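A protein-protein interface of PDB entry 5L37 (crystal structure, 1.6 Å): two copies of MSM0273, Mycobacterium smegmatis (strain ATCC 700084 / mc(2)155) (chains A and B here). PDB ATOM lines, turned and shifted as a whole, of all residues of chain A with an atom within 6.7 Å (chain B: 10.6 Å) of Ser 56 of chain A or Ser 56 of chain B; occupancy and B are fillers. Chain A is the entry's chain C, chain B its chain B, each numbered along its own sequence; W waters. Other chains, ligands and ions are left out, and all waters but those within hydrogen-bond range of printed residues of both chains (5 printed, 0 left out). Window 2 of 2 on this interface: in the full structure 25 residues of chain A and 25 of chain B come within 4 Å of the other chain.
Ser 56 of chain B touches Ser 56 of chain A (CB to OG, 3.5 Å). Val 57 of chain A touches Ser 56 of chain B (CG1 to CA, 3.8 Å). Ser 59 of chain B touches Val 57 of chain A (CB to CG1, 3.5 Å). Val 57 of chain A touches Ile 69 of chain B (CG1 to O, 3.5 Å). Val 57 of chain A touches Asp 70 of chain B (CG2 to CB, 3.98 Å). Trp 61 of chain A touches Pro 68 of chain B (CD1 to CG, 3.8 Å).
Water W3 lies within hydrogen-bond range of OG of Ser 60 of chain A and OG of Ser 59 of chain B. Water W1 bridges the backbone carbonyl oxygen of Pro 66 of chain B (2.6 Å) and the backbone carbonyl oxygen of Ser 60 of chain A (2.8 Å). Water W5 lies within hydrogen-bond range of OD2 of Asp 70 of chain B (2.7 Å) and OE1 of Gln 54 of chain A (2.8 Å). Water W2 lies within hydrogen-bond range of the side-chain hydroxyl (OG) of Ser 60 of chain A (2.7 Å), the backbone carbonyl oxygen (O) of Val 57 of chain A (2.8 Å), the backbone NH (N) of Trp 61 of chain A (3.1 Å) and the backbone carbonyl oxygen (O) of Pro 66 of chain B (3.2 Å). Water W4 lies within hydrogen-bond range of O of Gln 54 of chain A and OD2 of Asp 70 of chain B.
Printed residues of chain B that touch a printed residue of chain A: Ser 56, Ser 59, Pro 68, Ile 69 and Asp 70. Of the 10 printed residues of chain A, 4 touch a printed residue of chain B. Printed residues of chain A that touch a printed residue of chain B: Gln 54, Ser 56, Val 57 and Trp 61. Hydrophobic or aromatic side chains of chain A that line the printed part of chain B: Val 57 and Trp 61. Along chain A the printed residues that touch a printed residue of chain B span positions 54 to 61. Among the printed residues, 7 pairs touch across the chains.
Gln 54 of chain A touches Asp 70 of chain B, but with the chains exchanged Asp 70 of chain A does not touch Gln 54 of chain B (11.7 Å). Val 57 of chain A touches Ser 56 of chain B, but with the chains exchanged Ser 56 of chain A does not touch Val 57 of chain B (6.9 Å). Val 57 of chain A touches Ser 59 of chain B, but with the chains exchanged Ser 59 of chain A does not touch Val 57 of chain B (12.2 Å). Val 57 of chain A touches Asp 70 of chain B, but with the chains exchanged Asp 70 of chain A does not touch Val 57 of chain B (13.1 Å).
Printed residues of chain B within 4 Å of Ser 56 of chain A: Ser 56 (3.5 Å). Ser 56 of chain B touches two residues of chain A. No residue of chain B comes within 4 Å of Gly 55 of chain A. No residue of chain B comes within 4 Å of Ala 58 of chain A. No residue of chain B comes within 4 Å of Ser 59 of chain A. No residue of chain B comes within 4 Å of Ser 60 of chain A. Of the printed residues of chain A, Pro 68 of chain B touches Trp 61 (3.8 Å). Printed residues of chain A within 4 Å of Ile 69 of chain B: Val 57. Printed residues of chain A within 4 Å of Ser 59 of chain B: Val 57. Of the printed residues of chain B, Trp 61 of chain A touches Pro 68. Printed residues of chain A within 4 Å of Asp 70 of chain B: Gln 54 and Val 57. Ala 71 of chain B touches none of the printed residues of chain A. The nearest residue of chain B that does not touch Ser 56 of chain A is Gly 55 of chain B (6.0 Å).
N of Gly 55 of chain B is in hydrogen-bond range of O of Asp 70 of chain B (2.8 Å). O of Ser 56 of chain B sits at hydrogen-bond distance from OG of Ser 60 of chain B (3.3 Å). OG of Ser 59 of chain B sits at hydrogen-bond distance from O of Pro 67 of chain B, at 2.7 Å. O of Ser 56 of chain A is in hydrogen-bond range of OG of Ser 60 of chain A, at 3.4 Å. The backbone carbonyl oxygen of Val 57 of chain A sits at hydrogen-bond distance from the side-chain hydroxyl of Ser 60 of chain A, 3.4 Å away.
N of Gln 54 of chain A sits at hydrogen-bond distance from OD2 of Asp 70 of chain B (2.8 Å).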
ATOM      1  N   GLN A  54      10.937   9.829  22.131  1.00  0.00           N
ATOM      2  CA  GLN A  54       9.744  10.148  22.941  1.00  0.00           C
ATOM      3  C   GLN A  54       8.761   9.001  23.003  1.00  0.00           C
ATOM      4  O   GLN A  54       8.743   8.107  22.131  1.00  0.00           O
ATOM      5  CB  GLN A  54       9.036  11.358  22.346  1.00  0.00           C
ATOM      6  CG  GLN A  54       9.887  12.628  22.384  1.00  0.00           C
ATOM      7  CD  GLN A  54       9.153  13.770  21.736  1.00  0.00           C
ATOM      8  OE1 GLN A  54       9.248  13.983  20.532  1.00  0.00           O
ATOM      9  NE2 GLN A  54       8.343  14.465  22.524  1.00  0.00           N
ATOM     10  N   GLY A  55       7.902   9.049  24.011  1.00  0.00           N
ATOM     11  CA  GLY A  55       6.844   8.044  24.129  1.00  0.00           C
ATOM     12  C   GLY A  55       7.290   6.850  24.934  1.00  0.00           C
ATOM     13  O   GLY A  55       8.265   6.903  25.729  1.00  0.00           O
ATOM     14  N   SER A  56       6.576   5.730  24.746  1.00  0.00           N
ATOM     15  CA  SER A  56       6.815   4.570  25.582  1.00  0.00           C
ATOM     16  C   SER A  56       8.196   3.966  25.318  1.00  0.00           C
ATOM     17  O   SER A  56       8.716   3.274  26.209  1.00  0.00           O
ATOM     18  CB  SER A  56       5.717   3.526  25.414  1.00  0.00           C
ATOM     19  OG  SER A  56       5.717   3.058  24.107  1.00  0.00           O
ATOM     20  N   VAL A  57       8.805   4.236  24.162  1.00  0.00           N
ATOM     21  CA  VAL A  57      10.140   3.669  23.926  1.00  0.00           C
ATOM     22  C   VAL A  57      11.178   4.291  24.873  1.00  0.00           C
ATOM     23  O   VAL A  57      12.199   3.652  25.159  1.00  0.00           O
ATOM     24  CB  VAL A  57      10.614   3.825  22.452  1.00  0.00           C
ATOM     25  CG1 VAL A  57       9.543   3.258  21.478  1.00  0.00           C
ATOM     26  CG2 VAL A  57      10.985   5.260  22.110  1.00  0.00           C
ATOM     27  N   ALA A  58      10.914   5.492  25.380  1.00  0.00           N
ATOM     28  CA  ALA A  58      11.827   6.084  26.381  1.00  0.00           C
ATOM     29  C   ALA A  58      11.825   5.292  27.687  1.00  0.00           C
ATOM     30  O   ALA A  58      12.868   4.945  28.222  1.00  0.00           O
ATOM     31  CB  ALA A  58      11.440   7.557  26.638  1.00  0.00           C
ATOM     32  N   SER A  59      10.653   4.836  28.101  1.00  0.00           N
ATOM     33  CA  SER A  59      10.515   4.064  29.325  1.00  0.00           C
ATOM     34  C   SER A  59      11.025   2.625  29.110  1.00  0.00           C
ATOM     35  O   SER A  59      11.652   2.021  29.999  1.00  0.00           O
ATOM     36  CB  SER A  59       9.020   4.078  29.731  1.00  0.00           C
ATOM     37  OG  SER A  59       8.701   3.148  30.750  1.00  0.00           O
ATOM     38  N   SER A  60      10.740   2.043  27.951  1.00  0.00           N
ATOM     39  CA  SER A  60      11.057   0.633  27.791  1.00  0.00           C
ATOM     40  C   SER A  60      12.564   0.364  27.684  1.00  0.00           C
ATOM     41  O   SER A  60      12.975  -0.795  27.742  1.00  0.00           O
ATOM     42  CB  SER A  60      10.295   0.040  26.586  1.00  0.00           C
ATOM     43  OG  SER A  60      10.709   0.598  25.349  1.00  0.00           O
ATOM     44  N   TRP A  61      13.371   1.411  27.535  1.00  0.00           N
ATOM     45  CA  TRP A  61      14.843   1.241  27.526  1.00  0.00           C
ATOM     46  C   TRP A  61      15.354   0.725  28.865  1.00  0.00           C
ATOM     47  O   TRP A  61      16.353  -0.021  28.941  1.00  0.00           O
ATOM     48  CB  TRP A  61      15.554   2.566  27.181  1.00  0.00           C
ATOM     49  CG  TRP A  61      17.071   2.449  27.138  1.00  0.00           C
ATOM     50  CD1 TRP A  61      17.835   1.963  26.095  1.00  0.00           C
ATOM     51  CD2 TRP A  61      17.993   2.799  28.182  1.00  0.00           C
ATOM     52  NE1 TRP A  61      19.179   1.979  26.436  1.00  0.00           N
ATOM     53  CE2 TRP A  61      19.307   2.511  27.704  1.00  0.00           C
ATOM     54  CE3 TRP A  61      17.853   3.335  29.470  1.00  0.00           C
ATOM     55  CZ2 TRP A  61      20.451   2.733  28.459  1.00  0.00           C
ATOM     56  CZ3 TRP A  61      19.008   3.564  30.225  1.00  0.00           C
ATOM     57  CH2 TRP A  61      20.288   3.251  29.716  1.00  0.00           C
ATOM     58  N   ILE A  69       8.466   7.725  32.272  1.00  0.00           N
ATOM     59  CA  ILE A  69       9.331   8.627  31.516  1.00  0.00           C
ATOM     60  C   ILE A  69       8.915   8.555  30.056  1.00  0.00           C
ATOM     61  O   ILE A  69       8.869   7.434  29.488  1.00  0.00           O
ATOM     62  CB  ILE A  69      10.817   8.170  31.677  1.00  0.00           C
ATOM     63  CG1 ILE A  69      11.235   8.318  33.141  1.00  0.00           C
ATOM     64  CG2 ILE A  69      11.748   8.924  30.729  1.00  0.00           C
ATOM     65  CD1 ILE A  69      11.209   9.738  33.601  1.00  0.00           C
ATOM     66  N   ASP A  70       8.639   9.714  29.439  1.00  0.00           N
ATOM     67  CA  ASP A  70       8.174   9.750  28.035  1.00  0.00           C
ATOM     68  C   ASP A  70       9.145  10.542  27.105  1.00  0.00           C
ATOM     69  O   ASP A  70       8.785  10.899  25.980  1.00  0.00           O
ATOM     70  CB  ASP A  70       6.747  10.356  27.986  1.00  0.00           C
ATOM     71  CG  ASP A  70       6.710  11.852  28.393  1.00  0.00           C
ATOM     72  OD1 ASP A  70       7.793  12.407  28.621  1.00  0.00           O
ATOM     73  OD2 ASP A  70       5.610  12.452  28.426  1.00  0.00           O
ATOM     74  N   ALA B  53       7.114   5.684   9.871  1.00  0.00           N
ATOM     75  CA  ALA B  53       6.199   5.348  10.976  1.00  0.00           C
ATOM     76  C   ALA B  53       6.782   5.825  12.296  1.00  0.00           C
ATOM     77  O   ALA B  53       8.010   5.803  12.497  1.00  0.00           O
ATOM     78  CB  ALA B  53       5.906   3.824  11.010  1.00  0.00           C
ATOM     79  N   GLN B  54       5.904   6.249  13.206  1.00  0.00           N
ATOM     80  CA  GLN B  54       6.325   6.863  14.476  1.00  0.00           C
ATOM     81  C   GLN B  54       5.767   6.118  15.685  1.00  0.00           C
ATOM     82  O   GLN B  54       4.722   5.454  15.610  1.00  0.00           O
ATOM     83  CB  GLN B  54       5.862   8.338  14.532  1.00  0.00           C
ATOM     84  CG  GLN B  54       6.531   9.195  13.463  1.00  0.00           C
ATOM     85  CD  GLN B  54       6.006  10.599  13.500  1.00  0.00           C
ATOM     86  OE1 GLN B  54       4.959  10.891  12.909  1.00  0.00           O
ATOM     87  NE2 GLN B  54       6.659  11.465  14.277  1.00  0.00           N
ATOM     88  N   GLY B  55       6.437   6.337  16.826  1.00  0.00           N
ATOM     89  CA  GLY B  55       5.985   5.807  18.093  1.00  0.00           C
ATOM     90  C   GLY B  55       6.519   4.417  18.324  1.00  0.00           C
ATOM     91  O   GLY B  55       7.528   4.010  17.758  1.00  0.00           O
ATOM     92  N   SER B  56       5.814   3.687  19.175  1.00  0.00           N
ATOM     93  CA  SER B  56       6.331   2.410  19.644  1.00  0.00           C
ATOM     94  C   SER B  56       6.426   1.363  18.522  1.00  0.00           C
ATOM     95  O   SER B  56       7.240   0.474  18.643  1.00  0.00           O
ATOM     96  CB  SER B  56       5.494   1.879  20.808  1.00  0.00           C
ATOM     97  OG  SER B  56       4.181   1.575  20.397  1.00  0.00           O
ATOM     98  N   VAL B  57       5.667   1.495  17.429  1.00  0.00           N
ATOM     99  CA  VAL B  57       5.780   0.497  16.367  1.00  0.00           C
ATOM    100  C   VAL B  57       7.142   0.584  15.685  1.00  0.00           C
ATOM    101  O   VAL B  57       7.583  -0.390  15.069  1.00  0.00           O
ATOM    102  CB  VAL B  57       4.615   0.625  15.329  1.00  0.00           C
ATOM    103  CG1 VAL B  57       3.261   0.579  16.045  1.00  0.00           C
ATOM    104  CG2 VAL B  57       4.736   1.882  14.471  1.00  0.00           C
ATOM    105  N   ALA B  58       7.810   1.731  15.750  1.00  0.00           N
ATOM    106  CA  ALA B  58       9.156   1.821  15.190  1.00  0.00           C
ATOM    107  C   ALA B  58      10.135   0.943  16.004  1.00  0.00           C
ATOM    108  O   ALA B  58      11.102   0.456  15.472  1.00  0.00           O
ATOM    109  CB  ALA B  58       9.652   3.300  15.172  1.00  0.00           C
ATOM    110  N   SER B  59       9.923   0.839  17.300  1.00  0.00           N
ATOM    111  CA  SER B  59      10.802   0.028  18.157  1.00  0.00           C
ATOM    112  C   SER B  59      10.414  -1.451  18.099  1.00  0.00           C
ATOM    113  O   SER B  59      11.277  -2.351  18.041  1.00  0.00           O
ATOM    114  CB  SER B  59      10.701   0.561  19.592  1.00  0.00           C
ATOM    115  OG  SER B  59      11.364  -0.281  20.536  1.00  0.00           O
ATOM    116  N   SER B  60       9.109  -1.728  18.118  1.00  0.00           N
ATOM    117  CA  SER B  60       8.711  -3.122  18.205  1.00  0.00           C
ATOM    118  C   SER B  60       8.981  -3.919  16.925  1.00  0.00           C
ATOM    119  O   SER B  60       8.938  -5.145  16.950  1.00  0.00           O
ATOM    120  CB  SER B  60       7.227  -3.212  18.644  1.00  0.00           C
ATOM    121  OG  SER B  60       6.428  -2.591  17.668  1.00  0.00           O
ATOM    122  N   TRP B  61       9.309  -3.244  15.832  1.00  0.00           N
ATOM    123  CA  TRP B  61       9.666  -3.951  14.593  1.00  0.00           C
ATOM    124  C   TRP B  61      10.937  -4.793  14.743  1.00  0.00           C
ATOM    125  O   TRP B  61      11.097  -5.849  14.097  1.00  0.00           O
ATOM    126  CB  TRP B  61       9.882  -2.931  13.473  1.00  0.00           C
ATOM    127  CG  TRP B  61      10.198  -3.587  12.168  1.00  0.00           C
ATOM    128  CD1 TRP B  61       9.291  -4.146  11.292  1.00  0.00           C
ATOM    129  CD2 TRP B  61      11.506  -3.795  11.580  1.00  0.00           C
ATOM    130  NE1 TRP B  61       9.935  -4.710  10.242  1.00  0.00           N
ATOM    131  CE2 TRP B  61      11.283  -4.504  10.366  1.00  0.00           C
ATOM    132  CE3 TRP B  61      12.821  -3.486  11.967  1.00  0.00           C
ATOM    133  CZ2 TRP B  61      12.338  -4.886   9.527  1.00  0.00           C
ATOM    134  CZ3 TRP B  61      13.873  -3.851  11.131  1.00  0.00           C
ATOM    135  CH2 TRP B  61      13.609  -4.566   9.908  1.00  0.00           C
ATOM    136  N   PHE B  62      11.859  -4.311  15.580  1.00  0.00           N
ATOM    137  CA  PHE B  62      13.165  -4.959  15.724  1.00  0.00           C
ATOM    138  C   PHE B  62      13.143  -6.220  16.560  1.00  0.00           C
ATOM    139  O   PHE B  62      12.339  -6.343  17.497  1.00  0.00           O
ATOM    140  CB  PHE B  62      14.167  -3.970  16.364  1.00  0.00           C
ATOM    141  CG  PHE B  62      14.514  -2.839  15.464  1.00  0.00           C
ATOM    142  CD1 PHE B  62      15.578  -2.962  14.588  1.00  0.00           C
ATOM    143  CD2 PHE B  62      13.728  -1.695  15.410  1.00  0.00           C
ATOM    144  CE1 PHE B  62      15.905  -1.955  13.677  1.00  0.00           C
ATOM    145  CE2 PHE B  62      14.048  -0.655  14.522  1.00  0.00           C
ATOM    146  CZ  PHE B  62      15.147  -0.804  13.626  1.00  0.00           C
ATOM    147  N   THR B  63      13.992  -7.172  16.164  1.00  0.00           N
ATOM    148  CA  THR B  63      14.261  -8.341  16.970  1.00  0.00           C
ATOM    149  C   THR B  63      15.265  -7.921  18.049  1.00  0.00           C
ATOM    150  O   THR B  63      15.861  -6.842  17.982  1.00  0.00           O
ATOM    151  CB  THR B  63      14.916  -9.472  16.184  1.00  0.00           C
ATOM    152  OG1 THR B  63      16.112  -8.952  15.590  1.00  0.00           O
ATOM    153  CG2 THR B  63      13.971  -9.998  15.121  1.00  0.00           C
ATOM    154  N   THR B  65      16.263  -6.863  21.999  1.00  0.00           N
ATOM    155  CA  THR B  65      15.702  -5.916  22.939  1.00  0.00           C
ATOM    156  C   THR B  65      15.174  -4.695  22.175  1.00  0.00           C
ATOM    157  O   THR B  65      15.934  -4.071  21.467  1.00  0.00           O
ATOM    158  CB  THR B  65      16.783  -5.480  23.947  1.00  0.00           C
ATOM    159  OG1 THR B  65      17.340  -6.662  24.559  1.00  0.00           O
ATOM    160  CG2 THR B  65      16.210  -4.563  25.019  1.00  0.00           C
ATOM    161  N   PRO B  66      13.906  -4.333  22.388  1.00  0.00           N
ATOM    162  CA  PRO B  66      13.318  -3.217  21.629  1.00  0.00           C
ATOM    163  C   PRO B  66      14.081  -1.914  21.915  1.00  0.00           C
ATOM    164  O   PRO B  66      14.240  -1.591  23.074  1.00  0.00           O
ATOM    165  CB  PRO B  66      11.857  -3.187  22.117  1.00  0.00           C
ATOM    166  CG  PRO B  66      11.845  -3.969  23.407  1.00  0.00           C
ATOM    167  CD  PRO B  66      12.911  -5.024  23.230  1.00  0.00           C
ATOM    168  N   PRO B  67      14.628  -1.276  20.868  1.00  0.00           N
ATOM    169  CA  PRO B  67      15.508  -0.098  20.942  1.00  0.00           C
ATOM    170  C   PRO B  67      14.755   1.183  21.199  1.00  0.00           C
ATOM    171  O   PRO B  67      13.556   1.295  20.937  1.00  0.00           O
ATOM    172  CB  PRO B  67      16.182  -0.050  19.583  1.00  0.00           C
ATOM    173  CG  PRO B  67      15.116  -0.668  18.658  1.00  0.00           C
ATOM    174  CD  PRO B  67      14.434  -1.716  19.469  1.00  0.00           C
ATOM    175  N   PRO B  68      15.473   2.181  21.716  1.00  0.00           N
ATOM    176  CA  PRO B  68      14.844   3.464  22.048  1.00  0.00           C
ATOM    177  C   PRO B  68      14.717   4.349  20.803  1.00  0.00           C
ATOM    178  O   PRO B  68      15.292   5.435  20.694  1.00  0.00           O
ATOM    179  CB  PRO B  68      15.805   4.055  23.100  1.00  0.00           C
ATOM    180  CG  PRO B  68      17.092   3.558  22.682  1.00  0.00           C
ATOM    181  CD  PRO B  68      16.890   2.135  22.131  1.00  0.00           C
ATOM    182  N   ILE B  69      13.902   3.858  19.881  1.00  0.00           N
ATOM    183  CA  ILE B  69      13.726   4.461  18.577  1.00  0.00           C
ATOM    184  C   ILE B  69      12.216   4.726  18.380  1.00  0.00           C
ATOM    185  O   ILE B  69      11.389   3.782  18.512  1.00  0.00           O
ATOM    186  CB  ILE B  69      14.242   3.473  17.476  1.00  0.00           C
ATOM    187  CG1 ILE B  69      15.755   3.262  17.593  1.00  0.00           C
ATOM    188  CG2 ILE B  69      13.828   3.906  16.081  1.00  0.00           C
ATOM    189  CD1 ILE B  69      16.524   4.517  17.386  1.00  0.00           C
ATOM    190  N   ASP B  70      11.857   5.965  18.016  1.00  0.00           N
ATOM    191  CA  ASP B  70      10.416   6.314  17.858  1.00  0.00           C
ATOM    192  C   ASP B  70      10.047   6.799  16.452  1.00  0.00           C
ATOM    193  O   ASP B  70       8.999   7.376  16.275  1.00  0.00           O
ATOM    194  CB  ASP B  70      10.021   7.386  18.883  1.00  0.00           C
ATOM    195  CG  ASP B  70      10.764   8.693  18.665  1.00  0.00           C
ATOM    196  OD1 ASP B  70      11.549   8.770  17.709  1.00  0.00           O
ATOM    197  OD2 ASP B  70      10.525   9.671  19.403  1.00  0.00           O
ATOM    198  N   ALA B  71      10.934   6.552  15.482  1.00  0.00           N
ATOM    199  CA  ALA B  71      10.694   6.941  14.080  1.00  0.00           C
ATOM    200  C   ALA B  71      11.545   6.035  13.214  1.00  0.00           C
ATOM    201  O   ALA B  71      12.750   5.892  13.454  1.00  0.00           O
ATOM    202  CB  ALA B  71      11.054   8.417  13.834  1.00  0.00           C
ATOM    203  N   LEU B  72      10.873   5.394  12.242  1.00  0.00           N
ATOM    204  CA  LEU B  72      11.509   4.375  11.404  1.00  0.00           C
ATOM    205  C   LEU B  72      11.075   4.583   9.974  1.00  0.00           C
ATOM    206  O   LEU B  72       9.879   4.714   9.697  1.00  0.00           O
ATOM    207  CB  LEU B  72      11.105   2.973  11.889  1.00  0.00           C
ATOM    208  CG  LEU B  72      11.627   1.773  11.084  1.00  0.00           C
ATOM    209  CD1 LEU B  72      13.180   1.673  11.141  1.00  0.00           C
ATOM    210  CD2 LEU B  72      11.016   0.466  11.639  1.00  0.00           C
ATOM    211  N   ILE B  74       9.991   3.107   6.829  1.00  0.00           N
ATOM    212  CA  ILE B  74       9.465   1.768   6.534  1.00  0.00           C
ATOM    213  C   ILE B  74       9.482   1.435   5.064  1.00  0.00           C
ATOM    214  O   ILE B  74       9.307   0.259   4.669  1.00  0.00           O
ATOM    215  CB  ILE B  74       8.036   1.586   7.094  1.00  0.00           C
ATOM    216  CG1 ILE B  74       7.013   2.486   6.370  1.00  0.00           C
ATOM    217  CG2 ILE B  74       8.054   1.815   8.620  1.00  0.00           C
ATOM    218  CD1 ILE B  74       5.555   2.215   6.812  1.00  0.00           C
HETATM  219  O   HOH W   1      13.479  -2.377  25.430  1.00  0.00           O
HETATM  220  O   HOH W   2      13.191   1.160  24.432  1.00  0.00           O
HETATM  221  O   HOH W   3      10.338  -0.071  23.067  1.00  0.00           O
HETATM  222  O   HOH W   4       7.104   9.182  19.659  1.00  0.00           O
HETATM  223  O   HOH W   5      10.849  12.277  18.917  1.00  0.00           O
